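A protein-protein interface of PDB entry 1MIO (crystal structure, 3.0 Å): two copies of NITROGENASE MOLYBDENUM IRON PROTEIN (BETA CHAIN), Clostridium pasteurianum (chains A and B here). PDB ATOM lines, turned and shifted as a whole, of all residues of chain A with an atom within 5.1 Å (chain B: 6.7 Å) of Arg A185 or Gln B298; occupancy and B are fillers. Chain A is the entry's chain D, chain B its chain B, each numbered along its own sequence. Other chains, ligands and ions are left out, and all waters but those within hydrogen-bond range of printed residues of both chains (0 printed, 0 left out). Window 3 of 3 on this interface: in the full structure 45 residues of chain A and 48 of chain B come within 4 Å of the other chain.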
ATOM      1  N   PRO A 181      25.767   0.265 -21.398  1.00  0.00           N
ATOM      2  CA  PRO A 181      24.887  -0.675 -20.746  1.00  0.00           C
ATOM      3  C   PRO A 181      25.532  -1.576 -19.715  1.00  0.00           C
ATOM      4  O   PRO A 181      24.990  -1.683 -18.629  1.00  0.00           O
ATOM      5  CB  PRO A 181      24.247  -1.408 -21.917  1.00  0.00           C
ATOM      6  CG  PRO A 181      25.038  -1.090 -23.140  1.00  0.00           C
ATOM      7  CD  PRO A 181      25.466   0.324 -22.823  1.00  0.00           C
ATOM      8  N   ALA A 182      26.734  -2.077 -20.043  1.00  0.00           N
ATOM      9  CA  ALA A 182      27.588  -2.952 -19.240  1.00  0.00           C
ATOM     10  C   ALA A 182      28.099  -2.445 -17.894  1.00  0.00           C
ATOM     11  O   ALA A 182      28.316  -3.202 -16.932  1.00  0.00           O
ATOM     12  CB  ALA A 182      28.788  -3.342 -20.051  1.00  0.00           C
ATOM     13  N   ASP A 183      28.225  -1.122 -17.819  1.00  0.00           N
ATOM     14  CA  ASP A 183      28.672  -0.455 -16.617  1.00  0.00           C
ATOM     15  C   ASP A 183      27.498  -0.170 -15.702  1.00  0.00           C
ATOM     16  O   ASP A 183      27.625  -0.202 -14.495  1.00  0.00           O
ATOM     17  CB  ASP A 183      29.407   0.811 -17.042  1.00  0.00           C
ATOM     18  CG  ASP A 183      30.631   0.593 -17.934  1.00  0.00           C
ATOM     19  OD1 ASP A 183      31.139  -0.508 -18.099  1.00  0.00           O
ATOM     20  OD2 ASP A 183      31.114   1.556 -18.499  1.00  0.00           O
ATOM     21  N   MET A 184      26.320   0.064 -16.251  1.00  0.00           N
ATOM     22  CA  MET A 184      25.090   0.248 -15.514  1.00  0.00           C
ATOM     23  C   MET A 184      24.782  -1.115 -14.970  1.00  0.00           C
ATOM     24  O   MET A 184      24.669  -1.270 -13.763  1.00  0.00           O
ATOM     25  CB  MET A 184      23.988   0.743 -16.456  1.00  0.00           C
ATOM     26  CG  MET A 184      24.145   2.215 -16.730  1.00  0.00           C
ATOM     27  SD  MET A 184      23.592   2.741 -18.355  1.00  0.00           S
ATOM     28  CE  MET A 184      23.927   4.473 -18.389  1.00  0.00           C
ATOM     29  N   ARG A 185      24.758  -2.125 -15.816  1.00  0.00           N
ATOM     30  CA  ARG A 185      24.550  -3.506 -15.410  1.00  0.00           C
ATOM     31  C   ARG A 185      25.518  -3.982 -14.298  1.00  0.00           C
ATOM     32  O   ARG A 185      25.061  -4.632 -13.339  1.00  0.00           O
ATOM     33  CB  ARG A 185      24.667  -4.421 -16.667  1.00  0.00           C
ATOM     34  CG  ARG A 185      23.561  -4.170 -17.699  1.00  0.00           C
ATOM     35  CD  ARG A 185      23.576  -4.985 -18.993  1.00  0.00           C
ATOM     36  NE  ARG A 185      23.200  -6.393 -18.806  1.00  0.00           N
ATOM     37  CZ  ARG A 185      22.218  -7.054 -19.498  1.00  0.00           C
ATOM     38  NH1 ARG A 185      21.445  -6.477 -20.425  1.00  0.00           N
ATOM     39  NH2 ARG A 185      22.063  -8.383 -19.356  1.00  0.00           N
ATOM     40  N   GLU A 186      26.838  -3.666 -14.359  1.00  0.00           N
ATOM     41  CA  GLU A 186      27.826  -3.996 -13.325  1.00  0.00           C
ATOM     42  C   GLU A 186      27.526  -3.309 -12.023  1.00  0.00           C
ATOM     43  O   GLU A 186      27.677  -3.969 -10.981  1.00  0.00           O
ATOM     44  CB  GLU A 186      29.257  -3.582 -13.713  1.00  0.00           C
ATOM     45  CG  GLU A 186      30.356  -3.789 -12.631  1.00  0.00           C
ATOM     46  CD  GLU A 186      30.750  -5.196 -12.160  1.00  0.00           C
ATOM     47  OE1 GLU A 186      30.433  -6.180 -12.825  1.00  0.00           O
ATOM     48  OE2 GLU A 186      31.395  -5.293 -11.118  1.00  0.00           O
ATOM     49  N   ILE A 187      27.116  -2.016 -12.044  1.00  0.00           N
ATOM     50  CA  ILE A 187      26.851  -1.301 -10.783  1.00  0.00           C
ATOM     51  C   ILE A 187      25.593  -1.833 -10.097  1.00  0.00           C
ATOM     52  O   ILE A 187      25.566  -1.992  -8.875  1.00  0.00           O
ATOM     53  CB  ILE A 187      26.804   0.240 -11.064  1.00  0.00           C
ATOM     54  CG1 ILE A 187      28.191   0.722 -11.554  1.00  0.00           C
ATOM     55  CG2 ILE A 187      26.483   0.994  -9.772  1.00  0.00           C
ATOM     56  CD1 ILE A 187      28.241   2.073 -12.277  1.00  0.00           C
ATOM     57  N   LYS A 188      24.609  -2.262 -10.883  1.00  0.00           N
ATOM     58  CA  LYS A 188      23.428  -2.921 -10.349  1.00  0.00           C
ATOM     59  C   LYS A 188      23.821  -4.236  -9.689  1.00  0.00           C
ATOM     60  O   LYS A 188      23.389  -4.572  -8.582  1.00  0.00           O
ATOM     61  CB  LYS A 188      22.437  -3.127 -11.485  1.00  0.00           C
ATOM     62  CG  LYS A 188      21.976  -1.728 -11.818  1.00  0.00           C
ATOM     63  CD  LYS A 188      20.623  -1.650 -12.460  1.00  0.00           C
ATOM     64  CE  LYS A 188      20.531  -2.151 -13.878  1.00  0.00           C
ATOM     65  NZ  LYS A 188      19.153  -2.488 -14.161  1.00  0.00           N
ATOM     66  N   ARG A 189      24.761  -4.911 -10.323  1.00  0.00           N
ATOM     67  CA  ARG A 189      25.354  -6.130  -9.807  1.00  0.00           C
ATOM     68  C   ARG A 189      26.040  -5.946  -8.442  1.00  0.00           C
ATOM     69  O   ARG A 189      26.004  -6.815  -7.552  1.00  0.00           O
ATOM     70  CB  ARG A 189      26.312  -6.605 -10.873  1.00  0.00           C
ATOM     71  CG  ARG A 189      26.526  -8.080 -10.895  1.00  0.00           C
ATOM     72  CD  ARG A 189      27.651  -8.449  -9.973  1.00  0.00           C
ATOM     73  NE  ARG A 189      28.934  -8.133 -10.560  1.00  0.00           N
ATOM     74  CZ  ARG A 189      30.050  -8.542  -9.976  1.00  0.00           C
ATOM     75  NH1 ARG A 189      30.048  -9.254  -8.846  1.00  0.00           N
ATOM     76  NH2 ARG A 189      31.196  -8.163 -10.488  1.00  0.00           N
ATOM     77  N   SER A 205      20.822  -0.684 -19.953  1.00  0.00           N
ATOM     78  CA  SER A 205      20.935  -2.109 -19.792  1.00  0.00           C
ATOM     79  C   SER A 205      20.136  -2.987 -20.727  1.00  0.00           C
ATOM     80  O   SER A 205      20.768  -3.646 -21.523  1.00  0.00           O
ATOM     81  CB  SER A 205      20.558  -2.467 -18.391  1.00  0.00           C
ATOM     82  OG  SER A 205      21.141  -1.463 -17.588  1.00  0.00           O
ATOM     83  N   GLY A 206      18.809  -3.081 -20.764  1.00  0.00           N
ATOM     84  CA  GLY A 206      18.203  -3.993 -21.729  1.00  0.00           C
ATOM     85  C   GLY A 206      17.761  -3.316 -23.008  1.00  0.00           C
ATOM     86  O   GLY A 206      16.781  -3.755 -23.594  1.00  0.00           O
ATOM     87  N   ASP A 209      22.200  -3.171 -25.971  1.00  0.00           N
ATOM     88  CA  ASP A 209      22.827  -4.475 -26.056  1.00  0.00           C
ATOM     89  C   ASP A 209      21.612  -5.415 -26.065  1.00  0.00           C
ATOM     90  O   ASP A 209      20.436  -5.000 -26.090  1.00  0.00           O
ATOM     91  CB  ASP A 209      23.640  -4.817 -24.841  1.00  0.00           C
ATOM     92  CG  ASP A 209      22.837  -4.686 -23.562  1.00  0.00           C
ATOM     93  OD1 ASP A 209      22.385  -3.582 -23.308  1.00  0.00           O
ATOM     94  OD2 ASP A 209      22.659  -5.664 -22.848  1.00  0.00           O
ATOM     95  N   GLY A 210      21.817  -6.720 -26.070  1.00  0.00           N
ATOM     96  CA  GLY A 210      20.636  -7.536 -25.947  1.00  0.00           C
ATOM     97  C   GLY A 210      20.415  -8.504 -27.083  1.00  0.00           C
ATOM     98  O   GLY A 210      21.228  -8.581 -28.022  1.00  0.00           O
ATOM     99  N   PRO A 211      19.333  -9.282 -26.870  1.00  0.00           N
ATOM    100  CA  PRO A 211      19.077 -10.568 -27.477  1.00  0.00           C
ATOM    101  C   PRO A 211      18.577 -10.555 -28.882  1.00  0.00           C
ATOM    102  O   PRO A 211      17.733  -9.721 -29.130  1.00  0.00           O
ATOM    103  CB  PRO A 211      18.076 -11.243 -26.572  1.00  0.00           C
ATOM    104  CG  PRO A 211      18.092 -10.453 -25.296  1.00  0.00           C
ATOM    105  CD  PRO A 211      18.321  -9.059 -25.831  1.00  0.00           C
ATOM    106  N   THR A 212      19.013 -11.355 -29.836  1.00  0.00           N
ATOM    107  CA  THR A 212      18.241 -11.494 -31.040  1.00  0.00           C
ATOM    108  C   THR A 212      17.319 -12.633 -30.577  1.00  0.00           C
ATOM    109  O   THR A 212      17.838 -13.677 -30.153  1.00  0.00           O
ATOM    110  CB  THR A 212      19.174 -11.856 -32.210  1.00  0.00           C
ATOM    111  OG1 THR A 212      19.678 -10.615 -32.692  1.00  0.00           O
ATOM    112  CG2 THR A 212      18.500 -12.549 -33.348  1.00  0.00           C
ATOM    113  N   TYR A 421      29.659  -5.607 -23.780  1.00  0.00           N
ATOM    114  CA  TYR A 421      29.259  -6.609 -22.805  1.00  0.00           C
ATOM    115  C   TYR A 421      30.284  -6.645 -21.665  1.00  0.00           C
ATOM    116  O   TYR A 421      30.087  -7.297 -20.639  1.00  0.00           O
ATOM    117  CB  TYR A 421      29.134  -7.999 -23.489  1.00  0.00           C
ATOM    118  CG  TYR A 421      28.069  -8.236 -24.593  1.00  0.00           C
ATOM    119  CD1 TYR A 421      26.855  -7.558 -24.630  1.00  0.00           C
ATOM    120  CD2 TYR A 421      28.314  -9.147 -25.612  1.00  0.00           C
ATOM    121  CE1 TYR A 421      25.927  -7.783 -25.647  1.00  0.00           C
ATOM    122  CE2 TYR A 421      27.398  -9.378 -26.634  1.00  0.00           C
ATOM    123  CZ  TYR A 421      26.193  -8.691 -26.660  1.00  0.00           C
ATOM    124  OH  TYR A 421      25.268  -8.886 -27.692  1.00  0.00           O
ATOM    125  N   SER B 291      17.563 -14.753 -17.185  1.00  0.00           N
ATOM    126  CA  SER B 291      18.984 -14.410 -17.132  1.00  0.00           C
ATOM    127  C   SER B 291      19.785 -15.198 -18.170  1.00  0.00           C
ATOM    128  O   SER B 291      20.650 -14.694 -18.901  1.00  0.00           O
ATOM    129  CB  SER B 291      19.472 -14.693 -15.709  1.00  0.00           C
ATOM    130  OG  SER B 291      18.755 -15.757 -15.099  1.00  0.00           O
ATOM    131  N   GLU B 293      18.097 -17.000 -20.787  1.00  0.00           N
ATOM    132  CA  GLU B 293      17.498 -16.700 -22.113  1.00  0.00           C
ATOM    133  C   GLU B 293      18.169 -15.527 -22.828  1.00  0.00           C
ATOM    134  O   GLU B 293      18.257 -15.459 -24.067  1.00  0.00           O
ATOM    135  CB  GLU B 293      16.022 -16.263 -22.085  1.00  0.00           C
ATOM    136  CG  GLU B 293      14.953 -17.093 -21.392  1.00  0.00           C
ATOM    137  CD  GLU B 293      14.214 -18.102 -22.254  1.00  0.00           C
ATOM    138  OE1 GLU B 293      14.575 -18.298 -23.421  1.00  0.00           O
ATOM    139  OE2 GLU B 293      13.257 -18.706 -21.743  1.00  0.00           O
ATOM    140  N   GLU B 294      18.562 -14.584 -21.971  1.00  0.00           N
ATOM    141  CA  GLU B 294      19.167 -13.337 -22.354  1.00  0.00           C
ATOM    142  C   GLU B 294      20.647 -13.486 -22.622  1.00  0.00           C
ATOM    143  O   GLU B 294      21.107 -12.895 -23.604  1.00  0.00           O
ATOM    144  CB  GLU B 294      18.930 -12.322 -21.258  1.00  0.00           C
ATOM    145  CG  GLU B 294      19.411 -10.960 -21.711  1.00  0.00           C
ATOM    146  CD  GLU B 294      19.428  -9.824 -20.702  1.00  0.00           C
ATOM    147  OE1 GLU B 294      19.564 -10.056 -19.489  1.00  0.00           O
ATOM    148  OE2 GLU B 294      19.329  -8.685 -21.178  1.00  0.00           O
ATOM    149  N   GLU B 295      21.393 -14.238 -21.793  1.00  0.00           N
ATOM    150  CA  GLU B 295      22.798 -14.558 -22.074  1.00  0.00           C
ATOM    151  C   GLU B 295      22.816 -15.307 -23.406  1.00  0.00           C
ATOM    152  O   GLU B 295      23.675 -15.085 -24.266  1.00  0.00           O
ATOM    153  CB  GLU B 295      23.439 -15.496 -21.018  1.00  0.00           C
ATOM    154  CG  GLU B 295      24.113 -14.996 -19.718  1.00  0.00           C
ATOM    155  CD  GLU B 295      24.483 -16.096 -18.694  1.00  0.00           C
ATOM    156  OE1 GLU B 295      25.194 -17.057 -19.064  1.00  0.00           O
ATOM    157  OE2 GLU B 295      24.057 -15.971 -17.527  1.00  0.00           O
ATOM    158  N   ARG B 296      21.792 -16.154 -23.593  1.00  0.00           N
ATOM    159  CA  ARG B 296      21.643 -16.914 -24.805  1.00  0.00           C
ATOM    160  C   ARG B 296      21.348 -15.994 -25.982  1.00  0.00           C
ATOM    161  O   ARG B 296      21.947 -16.135 -27.052  1.00  0.00           O
ATOM    162  CB  ARG B 296      20.517 -17.912 -24.682  1.00  0.00           C
ATOM    163  CG  ARG B 296      20.706 -18.957 -25.800  1.00  0.00           C
ATOM    164  CD  ARG B 296      19.556 -19.965 -26.019  1.00  0.00           C
ATOM    165  NE  ARG B 296      19.818 -20.947 -27.081  1.00  0.00           N
ATOM    166  CZ  ARG B 296      19.605 -20.696 -28.377  1.00  0.00           C
ATOM    167  NH1 ARG B 296      19.141 -19.499 -28.764  1.00  0.00           N
ATOM    168  NH2 ARG B 296      19.820 -21.676 -29.267  1.00  0.00           N
ATOM    169  N   GLY B 297      20.449 -15.023 -25.825  1.00  0.00           N
ATOM    170  CA  GLY B 297      20.068 -14.141 -26.909  1.00  0.00           C
ATOM    171  C   GLY B 297      21.207 -13.288 -27.399  1.00  0.00           C
ATOM    172  O   GLY B 297      21.373 -13.064 -28.592  1.00  0.00           O
ATOM    173  N   GLN B 298      21.948 -12.769 -26.430  1.00  0.00           N
ATOM    174  CA  GLN B 298      23.105 -11.927 -26.668  1.00  0.00           C
ATOM    175  C   GLN B 298      24.180 -12.724 -27.368  1.00  0.00           C
ATOM    176  O   GLN B 298      24.868 -12.179 -28.218  1.00  0.00           O
ATOM    177  CB  GLN B 298      23.651 -11.395 -25.356  1.00  0.00           C
ATOM    178  CG  GLN B 298      22.681 -10.478 -24.622  1.00  0.00           C
ATOM    179  CD  GLN B 298      23.266  -9.906 -23.360  1.00  0.00           C
ATOM    180  OE1 GLN B 298      23.825 -10.581 -22.500  1.00  0.00           O
ATOM    181  NE2 GLN B 298      23.129  -8.600 -23.254  1.00  0.00           N
ATOM    182  N   LEU B 299      24.365 -13.997 -27.046  1.00  0.00           N
ATOM    183  CA  LEU B 299      25.284 -14.829 -27.791  1.00  0.00           C
ATOM    184  C   LEU B 299      24.870 -14.952 -29.265  1.00  0.00           C
ATOM    185  O   LEU B 299      25.682 -14.580 -30.126  1.00  0.00           O
ATOM    186  CB  LEU B 299      25.368 -16.211 -27.107  1.00  0.00           C
ATOM    187  CG  LEU B 299      26.173 -17.322 -27.751  1.00  0.00           C
ATOM    188  CD1 LEU B 299      27.573 -16.818 -27.997  1.00  0.00           C
ATOM    189  CD2 LEU B 299      26.128 -18.565 -26.910  1.00  0.00           C
ATOM    190  N   ILE B 300      23.640 -15.409 -29.595  1.00  0.00           N
ATOM    191  CA  ILE B 300      23.132 -15.555 -30.969  1.00  0.00           C
ATOM    192  C   ILE B 300      23.213 -14.213 -31.675  1.00  0.00           C
ATOM    193  O   ILE B 300      23.722 -14.126 -32.783  1.00  0.00           O
ATOM    194  CB  ILE B 300      21.680 -16.047 -30.970  1.00  0.00           C
ATOM    195  CG1 ILE B 300      21.591 -17.389 -30.267  1.00  0.00           C
ATOM    196  CG2 ILE B 300      21.163 -16.132 -32.395  1.00  0.00           C
ATOM    197  CD1 ILE B 300      22.227 -18.614 -30.924  1.00  0.00           C
ATOM    198  N   ASP B 301      22.813 -13.139 -31.049  1.00  0.00           N
ATOM    199  CA  ASP B 301      22.970 -11.835 -31.609  1.00  0.00           C
ATOM    200  C   ASP B 301      24.417 -11.530 -31.933  1.00  0.00           C
ATOM    201  O   ASP B 301      24.619 -10.923 -32.981  1.00  0.00           O
ATOM    202  CB  ASP B 301      22.420 -10.842 -30.620  1.00  0.00           C
ATOM    203  CG  ASP B 301      22.476  -9.395 -31.059  1.00  0.00           C
ATOM    204  OD1 ASP B 301      21.844  -9.002 -32.039  1.00  0.00           O
ATOM    205  OD2 ASP B 301      23.177  -8.651 -30.395  1.00  0.00           O
ATOM    206  N   LEU B 302      25.432 -11.880 -31.120  1.00  0.00           N
ATOM    207  CA  LEU B 302      26.853 -11.564 -31.371  1.00  0.00           C
ATOM    208  C   LEU B 302      27.383 -12.413 -32.490  1.00  0.00           C
ATOM    209  O   LEU B 302      28.128 -11.900 -33.320  1.00  0.00           O
ATOM    210  CB  LEU B 302      27.751 -11.798 -30.111  1.00  0.00           C
ATOM    211  CG  LEU B 302      29.291 -11.726 -30.091  1.00  0.00           C
ATOM    212  CD1 LEU B 302      29.849 -10.426 -30.601  1.00  0.00           C
ATOM    213  CD2 LEU B 302      29.704 -11.886 -28.685  1.00  0.00           C
ATOM    214  N   MET B 303      27.011 -13.683 -32.545  1.00  0.00           N
ATOM    215  CA  MET B 303      27.418 -14.525 -33.652  1.00  0.00           C
ATOM    216  C   MET B 303      26.783 -14.075 -34.973  1.00  0.00           C
ATOM    217  O   MET B 303      27.389 -14.309 -36.025  1.00  0.00           O
ATOM    218  CB  MET B 303      26.998 -15.937 -33.446  1.00  0.00           C
ATOM    219  CG  MET B 303      27.190 -16.585 -32.111  1.00  0.00           C
ATOM    220  SD  MET B 303      26.611 -18.268 -32.404  1.00  0.00           S
ATOM    221  CE  MET B 303      25.578 -18.370 -30.994  1.00  0.00           C
ATOM    222  N   ASP B 305      25.816 -10.679 -35.595  1.00  0.00           N
ATOM    223  CA  ASP B 305      26.475  -9.411 -35.979  1.00  0.00           C
ATOM    224  C   ASP B 305      27.907  -9.550 -36.555  1.00  0.00           C
ATOM    225  O   ASP B 305      28.264  -8.880 -37.531  1.00  0.00           O
ATOM    226  CB  ASP B 305      26.588  -8.440 -34.787  1.00  0.00           C
ATOM    227  CG  ASP B 305      25.317  -7.994 -34.095  1.00  0.00           C
ATOM    228  OD1 ASP B 305      24.239  -8.073 -34.684  1.00  0.00           O
ATOM    229  OD2 ASP B 305      25.445  -7.576 -32.946  1.00  0.00           O
ATOM    230  N   LYS B 428      28.379 -16.907 -21.619  1.00  0.00           N
ATOM    231  CA  LYS B 428      29.433 -15.935 -21.348  1.00  0.00           C
ATOM    232  C   LYS B 428      30.761 -16.192 -22.047  1.00  0.00           C
ATOM    233  O   LYS B 428      31.297 -15.359 -22.780  1.00  0.00           O
ATOM    234  CB  LYS B 428      29.670 -15.914 -19.870  1.00  0.00           C
ATOM    235  CG  LYS B 428      29.399 -14.580 -19.205  1.00  0.00           C
ATOM    236  CD  LYS B 428      27.942 -14.133 -18.944  1.00  0.00           C
ATOM    237  CE  LYS B 428      28.002 -13.004 -17.903  1.00  0.00           C
ATOM    238  NZ  LYS B 428      26.735 -12.808 -17.262  1.00  0.00           N
ATOM    239  N   ILE B 431      30.461 -15.889 -25.712  1.00  0.00           N
ATOM    240  CA  ILE B 431      30.449 -14.463 -26.113  1.00  0.00           C
ATOM    241  C   ILE B 431      31.886 -13.965 -26.194  1.00  0.00           C
ATOM    242  O   ILE B 431      32.349 -13.384 -27.170  1.00  0.00           O
ATOM    243  CB  ILE B 431      29.585 -13.656 -25.055  1.00  0.00           C
ATOM    244  CG1 ILE B 431      28.131 -13.925 -25.384  1.00  0.00           C
ATOM    245  CG2 ILE B 431      29.942 -12.170 -24.992  1.00  0.00           C
ATOM    246  CD1 ILE B 431      27.169 -13.506 -24.276  1.00  0.00           C
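No position is printed for both chains.
Of the 14 pairs that touch across the chains among the printed residues, none has its exchanged pair printed and touching as well.
NH1 of Arg A185 lies within hydrogen-bond range of O of Ser A205 (3.1 Å).
The side-chain carboxylate of Asp A209 lies within salt-bridge range of the guanidinium group of Arg A185 (2.8 Å).
O of Ser A205 lies close to OD1 of Asp A209, 2.4 Å away.
Gln B298 touches five residues of chain A.
Of the printed residues of chain B, Tyr A421 touches Gln B298 (3.4 Å), Asp B301 (3.4 Å), Leu B302 (3.98 Å) and Ile B431 (3.5 Å).
Of the printed residues of chain A, Leu B302 touches Tyr A421 (3.98 Å).
Printed residues of chain B within 4 Å of Thr A212: Gly B297 (3.2 Å) and Asp B301 (2.8 Å).
Arg B296 touches none of the printed residues of chain A.
Lys B428 touches none of the printed residues of chain A.
The nearest residue of chain A that does not touch Gln B298 is Thr A212 (4.7 Å).
The nearest printed residue of chain B that does not touch Tyr A421 is Leu B299 (5.2 Å).
Of the 15 printed residues of chain B, 6 touch a printed residue of chain A.
Printed residues of chain B that touch a printed residue of chain A: Glu B294, Gly B297, Gln B298, Asp B301, Leu B302 and Ile B431.
Hydrophobic or aromatic side chains of chain B that line the printed part of chain A: Leu B302 and Ile B431.
Hydrophobic or aromatic side chains of chain A within 4 Å of the printed part of chain B: Pro A211 and Tyr A421.
Among the printed residues, Asp or Glu carboxylates within 4 Å of a Lys or Arg side-chain nitrogen of the other chain: Arg A185 with Glu B294 (3.0 Å).
OE1 of Glu B294 lies within salt-bridge range of NH2 of Arg A185, at 3.0 Å.
O of Gly B297 sits at hydrogen-bond distance from N of Thr A212 (3.2 Å).
NE2 of Gln B298 lies within hydrogen-bond range of OD2 of Asp A209 (3.0 Å).
O of Gln B298 is in hydrogen-bond range of OH of Tyr A421, at 3.4 Å.
The side-chain hydroxyl (OG1) of Thr A212 lies within hydrogen-bond range of the side-chain carboxylate (OD1) of Asp B301 (2.8 Å).
The side-chain carboxylate (OD2) of Asp B301 sits close to the side-chain hydroxyl (OH) of Tyr A421 (3.4 Å).
The backbone carbonyl oxygen (O) of Gly A210 sits close to the side-chain carboxylate (OD2) of Asp B301, 3.1 Å away.
Gln B298 touches Arg A185 (NE2 to NH1, 3.9 Å).
N of Gly A210 touches NE2 of Gln B298 (3.6 Å).
Pro A211 touches Glu B294.
CA of Pro A211 touches C of Gly B297, 3.5 Å away.
Gln B298 touches Pro A211.
Leu B302 touches Tyr A421.
CD2 of Tyr A421 touches CG2 of Ile B431, 3.5 Å away.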
